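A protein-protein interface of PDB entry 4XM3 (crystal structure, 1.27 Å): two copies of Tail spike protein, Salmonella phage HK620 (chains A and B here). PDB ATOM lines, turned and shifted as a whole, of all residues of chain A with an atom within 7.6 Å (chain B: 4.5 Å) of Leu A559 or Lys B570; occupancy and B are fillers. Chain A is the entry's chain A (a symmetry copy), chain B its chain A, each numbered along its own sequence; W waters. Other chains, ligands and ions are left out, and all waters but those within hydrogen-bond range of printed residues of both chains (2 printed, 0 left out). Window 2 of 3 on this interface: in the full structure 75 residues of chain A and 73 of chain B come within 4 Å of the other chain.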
ATOM      1  N   ILE A 555      17.722   4.136   8.718  1.00  0.00           N
ATOM      2  CA  ILE A 555      17.578   5.587   8.363  1.00  0.00           C
ATOM      3  C   ILE A 555      16.213   5.845   7.741  1.00  0.00           C
ATOM      4  O   ILE A 555      15.529   4.950   7.242  1.00  0.00           O
ATOM      5  CB  ILE A 555      18.721   6.093   7.475  1.00  0.00           C
ATOM      6  CG1 ILE A 555      18.656   5.436   6.127  1.00  0.00           C
ATOM      7  CG2 ILE A 555      20.056   6.039   8.166  1.00  0.00           C
ATOM      8  CD1 ILE A 555      19.438   6.255   5.091  1.00  0.00           C
ATOM      9  N   ASN A 556      15.836   7.096   7.720  1.00  0.00           N
ATOM     10  CA  ASN A 556      14.581   7.534   7.073  1.00  0.00           C
ATOM     11  C   ASN A 556      14.913   8.319   5.819  1.00  0.00           C
ATOM     12  O   ASN A 556      15.390   9.471   5.913  1.00  0.00           O
ATOM     13  CB  ASN A 556      13.802   8.380   8.046  1.00  0.00           C
ATOM     14  CG  ASN A 556      12.571   9.006   7.436  1.00  0.00           C
ATOM     15  OD1 ASN A 556      11.887   8.391   6.631  1.00  0.00           O
ATOM     16  ND2 ASN A 556      12.282  10.246   7.835  1.00  0.00           N
ATOM     17  N   GLU A 557      14.575   7.730   4.681  1.00  0.00           N
ATOM     18  CA  GLU A 557      14.880   8.261   3.350  1.00  0.00           C
ATOM     19  C   GLU A 557      13.900   9.418   2.994  1.00  0.00           C
ATOM     20  O   GLU A 557      14.088  10.074   1.974  1.00  0.00           O
ATOM     21  CB  GLU A 557      14.665   7.124   2.217  1.00  0.00           C
ATOM     22  CG  GLU A 557      13.101   7.142   1.897  1.00  0.00           C
ATOM     23  CD  GLU A 557      12.319   5.890   1.350  1.00  0.00           C
ATOM     24  OE1 GLU A 557      12.439   4.842   2.020  1.00  0.00           O
ATOM     25  OE2 GLU A 557      11.426   5.974   0.395  1.00  0.00           O
ATOM     26  N   ASN A 558      12.897   9.664   3.778  1.00  0.00           N
ATOM     27  CA  ASN A 558      11.819  10.613   3.447  1.00  0.00           C
ATOM     28  C   ASN A 558      12.109  11.990   3.935  1.00  0.00           C
ATOM     29  O   ASN A 558      12.781  12.148   4.993  1.00  0.00           O
ATOM     30  CB  ASN A 558      10.520  10.114   4.077  1.00  0.00           C
ATOM     31  CG  ASN A 558      10.117   8.774   3.490  1.00  0.00           C
ATOM     32  OD1 ASN A 558       9.667   8.693   2.369  1.00  0.00           O
ATOM     33  ND2 ASN A 558      10.410   7.703   4.219  1.00  0.00           N
ATOM     34  N   LEU A 559      11.590  12.996   3.233  1.00  0.00           N
ATOM     35  CA  LEU A 559      11.627  14.395   3.704  1.00  0.00           C
ATOM     36  C   LEU A 559      10.292  14.734   4.358  1.00  0.00           C
ATOM     37  O   LEU A 559      10.244  15.501   5.336  1.00  0.00           O
ATOM     38  CB  LEU A 559      11.871  15.361   2.530  1.00  0.00           C
ATOM     39  CG  LEU A 559      12.206  16.763   2.982  1.00  0.00           C
ATOM     40  CD1 LEU A 559      13.519  16.776   3.796  1.00  0.00           C
ATOM     41  CD2 LEU A 559      12.339  17.673   1.788  1.00  0.00           C
ATOM     42  N   ASP A 560       9.176  14.233   3.809  1.00  0.00           N
ATOM     43  CA  ASP A 560       7.844  14.740   4.252  1.00  0.00           C
ATOM     44  C   ASP A 560       7.297  14.132   5.501  1.00  0.00           C
ATOM     45  O   ASP A 560       6.238  14.577   5.953  1.00  0.00           O
ATOM     46  CB  ASP A 560       6.804  14.506   3.092  1.00  0.00           C
ATOM     47  CG  ASP A 560       7.074  15.302   1.841  1.00  0.00           C
ATOM     48  OD1 ASP A 560       8.009  16.163   1.803  1.00  0.00           O
ATOM     49  OD2 ASP A 560       6.291  15.058   0.859  1.00  0.00           O
ATOM     50  N   PHE A 561       7.941  13.117   6.019  1.00  0.00           N
ATOM     51  CA  PHE A 561       7.511  12.502   7.295  1.00  0.00           C
ATOM     52  C   PHE A 561       8.697  11.788   7.906  1.00  0.00           C
ATOM     53  O   PHE A 561       9.702  11.517   7.199  1.00  0.00           O
ATOM     54  CB  PHE A 561       6.320  11.537   7.099  1.00  0.00           C
ATOM     55  CG  PHE A 561       6.659  10.238   6.417  1.00  0.00           C
ATOM     56  CD1 PHE A 561       6.671  10.142   5.019  1.00  0.00           C
ATOM     57  CD2 PHE A 561       7.002   9.115   7.179  1.00  0.00           C
ATOM     58  CE1 PHE A 561       6.973   8.904   4.435  1.00  0.00           C
ATOM     59  CE2 PHE A 561       7.257   7.926   6.593  1.00  0.00           C
ATOM     60  CZ  PHE A 561       7.242   7.808   5.210  1.00  0.00           C
ATOM     61  N   SER A 562       8.448  11.358   9.131  1.00  0.00           N
ATOM     62  CA  SER A 562       9.386  10.483   9.786  1.00  0.00           C
ATOM     63  C   SER A 562       8.586   9.458  10.630  1.00  0.00           C
ATOM     64  O   SER A 562       7.593   9.811  11.264  1.00  0.00           O
ATOM     65  CB  SER A 562      10.368  11.251  10.667  1.00  0.00           C
ATOM     66  OG  SER A 562       9.685  12.076  11.592  1.00  0.00           O
ATOM     67  N   TYR A 580       5.933  11.744  12.730  1.00  0.00           N
ATOM     68  CA  TYR A 580       5.576  13.143  12.386  1.00  0.00           C
ATOM     69  C   TYR A 580       5.353  13.228  10.874  1.00  0.00           C
ATOM     70  O   TYR A 580       6.272  12.956  10.126  1.00  0.00           O
ATOM     71  CB  TYR A 580       6.666  14.160  12.817  1.00  0.00           C
ATOM     72  CG  TYR A 580       6.140  15.608  12.679  1.00  0.00           C
ATOM     73  CD1 TYR A 580       5.234  16.104  13.566  1.00  0.00           C
ATOM     74  CD2 TYR A 580       6.516  16.411  11.602  1.00  0.00           C
ATOM     75  CE1 TYR A 580       4.651  17.351  13.375  1.00  0.00           C
ATOM     76  CE2 TYR A 580       6.009  17.710  11.438  1.00  0.00           C
ATOM     77  CZ  TYR A 580       5.022  18.139  12.278  1.00  0.00           C
ATOM     78  OH  TYR A 580       4.399  19.398  12.170  1.00  0.00           O
ATOM     79  N   ASN A 581       4.173  13.719  10.494  1.00  0.00           N
ATOM     80  CA  ASN A 581       3.802  13.976   9.125  1.00  0.00           C
ATOM     81  C   ASN A 581       3.918  15.488   8.864  1.00  0.00           C
ATOM     82  O   ASN A 581       3.060  16.266   9.294  1.00  0.00           O
ATOM     83  CB  ASN A 581       2.337  13.561   8.854  1.00  0.00           C
ATOM     84  CG  ASN A 581       2.200  12.270   8.056  1.00  0.00           C
ATOM     85  OD1 ASN A 581       3.114  11.830   7.328  1.00  0.00           O
ATOM     86  ND2 ASN A 581       0.976  11.733   8.141  1.00  0.00           N
ATOM     87  N   GLU A 582       4.988  15.913   8.152  1.00  0.00           N
ATOM     88  CA  GLU A 582       5.080  17.331   7.784  1.00  0.00           C
ATOM     89  C   GLU A 582       3.918  17.740   6.905  1.00  0.00           C
ATOM     90  O   GLU A 582       3.293  18.769   7.095  1.00  0.00           O
ATOM     91  CB  GLU A 582       6.424  17.615   7.123  1.00  0.00           C
ATOM     92  CG  GLU A 582       6.564  19.021   6.631  1.00  0.00           C
ATOM     93  CD  GLU A 582       6.696  20.022   7.741  1.00  0.00           C
ATOM     94  OE1 GLU A 582       7.419  19.653   8.682  1.00  0.00           O
ATOM     95  OE2 GLU A 582       6.152  21.137   7.635  1.00  0.00           O
ATOM     96  N   ILE A 583       3.588  16.840   5.982  1.00  0.00           N
ATOM     97  CA  ILE A 583       2.400  16.837   5.159  1.00  0.00           C
ATOM     98  C   ILE A 583       1.636  15.588   5.521  1.00  0.00           C
ATOM     99  O   ILE A 583       2.225  14.605   5.791  1.00  0.00           O
ATOM    100  CB  ILE A 583       2.761  16.844   3.646  1.00  0.00           C
ATOM    101  CG1 ILE A 583       3.520  18.115   3.346  1.00  0.00           C
ATOM    102  CG2 ILE A 583       1.525  16.765   2.781  1.00  0.00           C
ATOM    103  CD1 ILE A 583       4.090  18.145   1.948  1.00  0.00           C
ATOM    104  N   ARG A 587       1.074   6.612   5.581  1.00  0.00           N
ATOM    105  CA  ARG A 587       2.435   6.205   5.258  1.00  0.00           C
ATOM    106  C   ARG A 587       2.585   4.710   5.478  1.00  0.00           C
ATOM    107  O   ARG A 587       1.895   4.134   6.354  1.00  0.00           O
ATOM    108  CB  ARG A 587       3.438   6.977   6.137  1.00  0.00           C
ATOM    109  CG  ARG A 587       3.277   8.458   6.171  1.00  0.00           C
ATOM    110  CD  ARG A 587       3.326   9.070   4.783  1.00  0.00           C
ATOM    111  NE  ARG A 587       3.328  10.517   4.904  1.00  0.00           N
ATOM    112  CZ  ARG A 587       3.577  11.353   3.907  1.00  0.00           C
ATOM    113  NH1 ARG A 587       3.921  10.869   2.700  1.00  0.00           N
ATOM    114  NH2 ARG A 587       3.606  12.674   4.128  1.00  0.00           N
ATOM    115  N   PHE B 538      13.696  19.954  15.261  1.00  0.00           N
ATOM    116  CA  PHE B 538      14.561  19.640  14.118  1.00  0.00           C
ATOM    117  C   PHE B 538      15.972  20.205  14.291  1.00  0.00           C
ATOM    118  O   PHE B 538      16.107  21.315  14.863  1.00  0.00           O
ATOM    119  CB  PHE B 538      14.038  20.283  12.802  1.00  0.00           C
ATOM    120  CG  PHE B 538      12.613  19.866  12.419  1.00  0.00           C
ATOM    121  CD1 PHE B 538      12.372  18.776  11.636  1.00  0.00           C
ATOM    122  CD2 PHE B 538      11.562  20.656  12.797  1.00  0.00           C
ATOM    123  CE1 PHE B 538      11.082  18.424  11.275  1.00  0.00           C
ATOM    124  CE2 PHE B 538      10.251  20.303  12.441  1.00  0.00           C
ATOM    125  CZ  PHE B 538      10.022  19.198  11.688  1.00  0.00           C
ATOM    126  N   ASN B 569      15.947  10.579  11.728  1.00  0.00           N
ATOM    127  CA  ASN B 569      16.425  11.544  10.783  1.00  0.00           C
ATOM    128  C   ASN B 569      15.426  11.807   9.655  1.00  0.00           C
ATOM    129  O   ASN B 569      14.379  11.180   9.594  1.00  0.00           O
ATOM    130  CB  ASN B 569      17.787  11.239  10.305  1.00  0.00           C
ATOM    131  CG  ASN B 569      17.857  10.119   9.369  1.00  0.00           C
ATOM    132  OD1 ASN B 569      16.954   9.213   9.237  1.00  0.00           O
ATOM    133  ND2 ASN B 569      19.054  10.028   8.828  1.00  0.00           N
ATOM    134  N   LYS B 570      15.814  12.661   8.729  1.00  0.00           N
ATOM    135  CA  LYS B 570      15.104  12.950   7.490  1.00  0.00           C
ATOM    136  C   LYS B 570      16.086  12.979   6.332  1.00  0.00           C
ATOM    137  O   LYS B 570      17.303  13.020   6.502  1.00  0.00           O
ATOM    138  CB  LYS B 570      14.527  14.389   7.489  1.00  0.00           C
ATOM    139  CG  LYS B 570      13.460  14.614   8.470  1.00  0.00           C
ATOM    140  CD  LYS B 570      13.144  16.133   8.655  1.00  0.00           C
ATOM    141  CE  LYS B 570      13.058  16.940   7.378  1.00  0.00           C
ATOM    142  NZ  LYS B 570      12.521  18.341   7.611  1.00  0.00           N
ATOM    143  N   ALA B 571      15.532  12.933   5.154  1.00  0.00           N
ATOM    144  CA  ALA B 571      16.352  12.831   3.927  1.00  0.00           C
ATOM    145  C   ALA B 571      17.369  13.930   3.757  1.00  0.00           C
ATOM    146  O   ALA B 571      18.386  13.742   3.113  1.00  0.00           O
ATOM    147  CB  ALA B 571      15.488  12.836   2.679  1.00  0.00           C
ATOM    148  N   ASN B 572      17.056  15.110   4.248  1.00  0.00           N
ATOM    149  CA  ASN B 572      17.985  16.246   4.116  1.00  0.00           C
ATOM    150  C   ASN B 572      19.088  16.268   5.123  1.00  0.00           C
ATOM    151  O   ASN B 572      19.911  17.215   5.118  1.00  0.00           O
ATOM    152  CB  ASN B 572      17.223  17.551   4.141  1.00  0.00           C
ATOM    153  CG  ASN B 572      16.590  17.825   5.489  1.00  0.00           C
ATOM    154  OD1 ASN B 572      16.578  16.981   6.384  1.00  0.00           O
ATOM    155  ND2 ASN B 572      16.027  18.981   5.630  1.00  0.00           N
ATOM    156  N   GLY B 573      19.151  15.254   5.990  1.00  0.00           N
ATOM    157  CA  GLY B 573      20.155  15.167   6.994  1.00  0.00           C
ATOM    158  C   GLY B 573      19.884  15.814   8.325  1.00  0.00           C
ATOM    159  O   GLY B 573      20.749  15.801   9.249  1.00  0.00           O
ATOM    160  N   GLN B 574      18.687  16.411   8.479  1.00  0.00           N
ATOM    161  CA  GLN B 574      18.252  16.823   9.814  1.00  0.00           C
ATOM    162  C   GLN B 574      17.813  15.648  10.704  1.00  0.00           C
ATOM    163  O   GLN B 574      17.350  14.620  10.219  1.00  0.00           O
ATOM    164  CB  GLN B 574      17.055  17.772   9.722  1.00  0.00           C
ATOM    165  CG  GLN B 574      17.340  19.099   9.116  1.00  0.00           C
ATOM    166  CD  GLN B 574      16.071  19.964   9.095  1.00  0.00           C
ATOM    167  OE1 GLN B 574      15.142  19.685   8.354  1.00  0.00           O
ATOM    168  NE2 GLN B 574      16.019  20.941   9.919  1.00  0.00           N
ATOM    169  N   VAL B 576      15.045  14.761  13.638  1.00  0.00           N
ATOM    170  CA  VAL B 576      13.629  15.126  13.978  1.00  0.00           C
ATOM    171  C   VAL B 576      13.130  14.263  15.120  1.00  0.00           C
ATOM    172  O   VAL B 576      13.370  13.053  15.141  1.00  0.00           O
ATOM    173  CB  VAL B 576      12.730  15.095  12.742  1.00  0.00           C
ATOM    174  CG1 VAL B 576      12.741  13.708  12.119  1.00  0.00           C
ATOM    175  CG2 VAL B 576      11.314  15.532  13.085  1.00  0.00           C
HETATM  176  O   HOH W   1       9.681  18.178   8.013  1.00  0.00           O
HETATM  177  O   HOH W   2      18.255   9.912   5.607  1.00  0.00           O
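The backbone carbonyl oxygen (O) of Asn A558 lies within hydrogen-bond range of the backbone NH (N) of Ala B571 (2.9 Å).
OD1 of Asn B569 sits at hydrogen-bond distance from N of Asn A556 (2.8 Å).
The side-chain amino group (NZ) of Lys B570 lies within hydrogen-bond range of the side-chain amide oxygen (OE1) of Gln B574, 3.0 Å away.
O of Tyr A580 is in hydrogen-bond range of N of Ser A562, at 2.9 Å.
ND2 of Asn B572 lies within hydrogen-bond range of OE1 of Gln B574 (2.9 Å).
The side-chain amide oxygen of Asn A556 is in hydrogen-bond range of the side-chain amide nitrogen of Asn A558 (2.9 Å).
ND2 of Asn A556 is in hydrogen-bond range of O of Phe A561 (2.9 Å).
Ile A555 touches Asn B569.
Asn A556 touches Lys B570 (O to C, 3.6 Å).
N of Ala B571 touches O of Asn A556 (3.5 Å).
CB of Ala B571 touches O of Glu A557 (3.2 Å).
Lys B570 touches Asn A558.
CE of Lys B570 touches CD1 of Leu A559, at 3.6 Å.
Leu A559 touches Ala B571 (N to CB, 3.9 Å).
CD1 of Leu A559 touches CG of Asn B572, at 3.7 Å.
Ser A562 touches Val B576 (OG to CG1, 3.5 Å).
Of the printed residues of chain B, Ile A555 touches Asn B569 (3.8 Å).
Of the printed residues of chain B, Ser A562 touches Val B576.
Tyr A580 touches none of the printed residues of chain B.
Printed residues of chain A within 4 Å of Asn B569: Ile A555 (3.8 Å) and Asn A556 (2.8 Å).
Of the printed residues of chain A, Ala B571 touches Asn A556 (3.5 Å), Glu A557 (3.2 Å), Asn A558 (2.9 Å) and Leu A559 (3.9 Å).
Gln B574 touches none of the printed residues of chain A.
Of the printed residues of chain A, Val B576 touches Ser A562 (3.5 Å).
The nearest printed residue of chain B that does not touch Glu A557 is Lys B570 (5.3 Å).
Printed residues of chain B that touch a printed residue of chain A: Asn B569, Lys B570, Ala B571, Asn B572 and Val B576.
Hydrophobic or aromatic side chains of chain B that line the printed part of chain A: Ala B571 and Val B576.
Hydrophobic or aromatic side chains of chain A within 4 Å of the printed part of chain B: Ile A555 and Leu A559.
Among the printed residues, 11 pairs touch across the chains.
Among the printed residues, no Asp or Glu carboxylate lies within 4 Å of a Lys or Arg side-chain nitrogen of the other chain.
No position is printed for both chains.
Water W1 bridges OE1 of Glu A582 (2.8 Å) and NZ of Lys B570 (2.9 Å).
Water W2 lies within hydrogen-bond range of O of Asn A556 (2.9 Å), ND2 of Asn B569 (3.3 Å) and O of Lys B570 (3.4 Å).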
